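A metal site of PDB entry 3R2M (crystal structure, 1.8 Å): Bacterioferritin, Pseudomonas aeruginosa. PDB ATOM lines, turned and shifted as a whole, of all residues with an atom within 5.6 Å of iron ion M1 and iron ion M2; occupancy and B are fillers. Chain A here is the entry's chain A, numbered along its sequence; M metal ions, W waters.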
ATOM      1  N   GLU A  18     -22.240 -19.893   5.740  1.00  0.00           N
ATOM      2  CA  GLU A  18     -21.469 -20.656   6.741  1.00  0.00           C
ATOM      3  C   GLU A  18     -20.049 -20.896   6.265  1.00  0.00           C
ATOM      4  O   GLU A  18     -19.098 -20.852   7.048  1.00  0.00           O
ATOM      5  CB  GLU A  18     -22.147 -22.017   7.037  1.00  0.00           C
ATOM      6  CG  GLU A  18     -23.533 -21.908   7.620  1.00  0.00           C
ATOM      7  CD  GLU A  18     -23.573 -21.153   8.915  1.00  0.00           C
ATOM      8  OE1 GLU A  18     -22.690 -21.376   9.756  1.00  0.00           O
ATOM      9  OE2 GLU A  18     -24.479 -20.328   9.105  1.00  0.00           O
ATOM     10  N   ALA A  21     -18.351 -17.679   7.025  1.00  0.00           N
ATOM     11  CA  ALA A  21     -18.074 -17.548   8.475  1.00  0.00           C
ATOM     12  C   ALA A  21     -16.826 -18.368   8.849  1.00  0.00           C
ATOM     13  O   ALA A  21     -15.929 -17.871   9.544  1.00  0.00           O
ATOM     14  CB  ALA A  21     -19.268 -18.039   9.283  1.00  0.00           C
ATOM     15  N   TYR A  25     -13.302 -16.679  10.293  1.00  0.00           N
ATOM     16  CA  TYR A  25     -12.651 -17.122  11.525  1.00  0.00           C
ATOM     17  C   TYR A  25     -11.270 -17.738  11.235  1.00  0.00           C
ATOM     18  O   TYR A  25     -10.374 -17.630  12.072  1.00  0.00           O
ATOM     19  CB  TYR A  25     -13.541 -18.160  12.221  1.00  0.00           C
ATOM     20  CG  TYR A  25     -14.765 -17.569  12.895  1.00  0.00           C
ATOM     21  CD1 TYR A  25     -14.658 -16.433  13.695  1.00  0.00           C
ATOM     22  CD2 TYR A  25     -16.010 -18.171  12.779  1.00  0.00           C
ATOM     23  CE1 TYR A  25     -15.760 -15.901  14.357  1.00  0.00           C
ATOM     24  CE2 TYR A  25     -17.122 -17.632  13.412  1.00  0.00           C
ATOM     25  CZ  TYR A  25     -16.983 -16.496  14.211  1.00  0.00           C
ATOM     26  OH  TYR A  25     -18.058 -15.961  14.895  1.00  0.00           O
ATOM     27  N   GLU A  50     -16.419 -25.155  14.271  1.00  0.00           N
ATOM     28  CA  GLU A  50     -17.874 -25.186  14.424  1.00  0.00           C
ATOM     29  C   GLU A  50     -18.645 -24.715  13.175  1.00  0.00           C
ATOM     30  O   GLU A  50     -19.665 -25.306  12.815  1.00  0.00           O
ATOM     31  CB  GLU A  50     -18.307 -24.373  15.642  1.00  0.00           C
ATOM     32  CG  GLU A  50     -17.853 -25.004  16.957  1.00  0.00           C
ATOM     33  CD  GLU A  50     -18.513 -24.407  18.164  1.00  0.00           C
ATOM     34  OE1 GLU A  50     -18.805 -23.197  18.159  1.00  0.00           O
ATOM     35  OE2 GLU A  50     -18.761 -25.149  19.139  1.00  0.00           O
ATOM     36  N   GLU A  51     -18.163 -23.661  12.517  1.00  0.00           N
ATOM     37  CA  GLU A  51     -18.817 -23.238  11.277  1.00  0.00           C
ATOM     38  C   GLU A  51     -18.605 -24.283  10.195  1.00  0.00           C
ATOM     39  O   GLU A  51     -19.465 -24.452   9.341  1.00  0.00           O
ATOM     40  CB  GLU A  51     -18.264 -21.909  10.760  1.00  0.00           C
ATOM     41  CG  GLU A  51     -18.332 -20.771  11.733  1.00  0.00           C
ATOM     42  CD  GLU A  51     -19.747 -20.385  12.152  1.00  0.00           C
ATOM     43  OE1 GLU A  51     -20.706 -20.957  11.654  1.00  0.00           O
ATOM     44  OE2 GLU A  51     -19.873 -19.481  12.986  1.00  0.00           O
ATOM     45  N   HIS A  54     -21.261 -26.618  10.851  1.00  0.00           N
ATOM     46  CA  HIS A  54     -22.549 -26.034  10.427  1.00  0.00           C
ATOM     47  C   HIS A  54     -22.728 -26.148   8.922  1.00  0.00           C
ATOM     48  O   HIS A  54     -23.763 -26.548   8.444  1.00  0.00           O
ATOM     49  CB  HIS A  54     -22.629 -24.554  10.834  1.00  0.00           C
ATOM     50  CG  HIS A  54     -22.889 -24.340  12.284  1.00  0.00           C
ATOM     51  ND1 HIS A  54     -22.940 -23.097  12.851  1.00  0.00           N
ATOM     52  CD2 HIS A  54     -23.116 -25.219  13.296  1.00  0.00           C
ATOM     53  CE1 HIS A  54     -23.184 -23.199  14.134  1.00  0.00           C
ATOM     54  NE2 HIS A  54     -23.303 -24.480  14.430  1.00  0.00           N
ATOM     55  N   GLU A  93     -22.211 -12.738  12.694  1.00  0.00           N
ATOM     56  CA  GLU A  93     -23.088 -13.639  13.457  1.00  0.00           C
ATOM     57  C   GLU A  93     -24.505 -13.082  13.543  1.00  0.00           C
ATOM     58  O   GLU A  93     -25.469 -13.843  13.519  1.00  0.00           O
ATOM     59  CB  GLU A  93     -22.543 -13.858  14.873  1.00  0.00           C
ATOM     60  CG  GLU A  93     -21.208 -14.640  14.866  1.00  0.00           C
ATOM     61  CD  GLU A  93     -21.415 -16.130  14.513  1.00  0.00           C
ATOM     62  OE1 GLU A  93     -22.537 -16.646  14.676  1.00  0.00           O
ATOM     63  OE2 GLU A  93     -20.426 -16.780  14.122  1.00  0.00           O
ATOM     64  N   VAL A  96     -26.067 -13.988  10.252  1.00  0.00           N
ATOM     65  CA  VAL A  96     -26.410 -15.404  10.317  1.00  0.00           C
ATOM     66  C   VAL A  96     -27.653 -15.659  11.193  1.00  0.00           C
ATOM     67  O   VAL A  96     -28.552 -16.411  10.787  1.00  0.00           O
ATOM     68  CB  VAL A  96     -25.209 -16.252  10.836  1.00  0.00           C
ATOM     69  CG1 VAL A  96     -25.683 -17.694  11.083  1.00  0.00           C
ATOM     70  CG2 VAL A  96     -24.089 -16.225   9.789  1.00  0.00           C
ATOM     71  N   LEU A 100     -30.928 -17.438   9.708  1.00  0.00           N
ATOM     72  CA  LEU A 100     -31.422 -18.705  10.241  1.00  0.00           C
ATOM     73  C   LEU A 100     -32.865 -18.566  10.713  1.00  0.00           C
ATOM     74  O   LEU A 100     -33.684 -19.462  10.495  1.00  0.00           O
ATOM     75  CB  LEU A 100     -30.517 -19.179  11.415  1.00  0.00           C
ATOM     76  CG  LEU A 100     -29.143 -19.735  11.004  1.00  0.00           C
ATOM     77  CD1 LEU A 100     -28.255 -19.833  12.243  1.00  0.00           C
ATOM     78  CD2 LEU A 100     -29.310 -21.113  10.321  1.00  0.00           C
ATOM     79  N   GLN A 122     -28.484 -24.749  14.847  1.00  0.00           N
ATOM     80  CA  GLN A 122     -27.504 -23.740  14.494  1.00  0.00           C
ATOM     81  C   GLN A 122     -27.823 -22.362  15.041  1.00  0.00           C
ATOM     82  O   GLN A 122     -26.920 -21.594  15.392  1.00  0.00           O
ATOM     83  CB  GLN A 122     -27.324 -23.699  12.983  1.00  0.00           C
ATOM     84  CG  GLN A 122     -26.778 -25.002  12.450  1.00  0.00           C
ATOM     85  CD  GLN A 122     -26.347 -24.891  10.998  1.00  0.00           C
ATOM     86  OE1 GLN A 122     -26.195 -23.801  10.456  1.00  0.00           O
ATOM     87  NE2 GLN A 122     -26.101 -26.035  10.379  1.00  0.00           N
ATOM     88  N   THR A 126     -25.439 -20.056  17.319  1.00  0.00           N
ATOM     89  CA  THR A 126     -25.166 -18.671  16.911  1.00  0.00           C
ATOM     90  C   THR A 126     -25.469 -17.654  18.036  1.00  0.00           C
ATOM     91  O   THR A 126     -24.669 -16.762  18.325  1.00  0.00           O
ATOM     92  CB  THR A 126     -26.004 -18.353  15.656  1.00  0.00           C
ATOM     93  OG1 THR A 126     -25.587 -19.223  14.586  1.00  0.00           O
ATOM     94  CG2 THR A 126     -25.862 -16.889  15.262  1.00  0.00           C
ATOM     95  N   HIS A 130     -21.658 -18.278  19.833  1.00  0.00           N
ATOM     96  CA  HIS A 130     -20.853 -17.386  18.978  1.00  0.00           C
ATOM     97  C   HIS A 130     -21.104 -15.893  19.218  1.00  0.00           C
ATOM     98  O   HIS A 130     -20.178 -15.147  19.542  1.00  0.00           O
ATOM     99  CB  HIS A 130     -21.114 -17.699  17.519  1.00  0.00           C
ATOM    100  CG  HIS A 130     -20.814 -19.123  17.140  1.00  0.00           C
ATOM    101  ND1 HIS A 130     -21.002 -19.618  15.874  1.00  0.00           N
ATOM    102  CD2 HIS A 130     -20.331 -20.154  17.881  1.00  0.00           C
ATOM    103  CE1 HIS A 130     -20.662 -20.891  15.839  1.00  0.00           C
ATOM    104  NE2 HIS A 130     -20.250 -21.240  17.046  1.00  0.00           N
HETATM  105 FE    FE M   1     -22.882 -21.005  11.855  1.00  0.00          FE
HETATM  106 FE    FE M   2     -21.533 -18.632  13.928  1.00  0.00          FE
HETATM  107  O   HOH W   1     -25.045 -21.011  11.615  1.00  0.00           O
HETATM  108  O   HOH W   2     -23.178 -19.564  13.340  1.00  0.00           O
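The nearest printed residue that does not touch iron ion M2 is Thr 126 (4.1 Å).
Iron ion M1 is bound by water W2, the side-chain carboxylate of Glu 18, water W1, the side-chain carboxylate of Glu 51 and a ring nitrogen (ND1) of His 54.
Water W2 is bound to iron ion M2 (2.0 Å).
The side-chain carboxylate (OE2) of Glu 51 binds iron ion M2, 2.1 Å away.
OE2 of Glu 93 is bound to iron ion M2 (2.2 Å).
ND1 of His 130 is bound to iron ion M2 (2.2 Å).
OE1 of Glu 93 is bound to iron ion M2 (2.3 Å).
OE2 of Glu 93 sits close to OH of Tyr 25.
NE2 of His 130 lies within hydrogen-bond range of OE1 of Glu 50 (2.7 Å).
The side-chain amide nitrogen (NE2) of Gln 122 sits at hydrogen-bond distance from the backbone carbonyl oxygen (O) of His 54 (3.1 Å).
Water W1 bridges OE2 of Glu 18 (2.7 Å) and OE1 of Gln 122 (3.2 Å).
Within 4 Å of iron ion M1: Glu 18, Glu 51 and His 54.
Along chain A the residues within 4 Å of iron ion M1 span positions 18 to 54.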
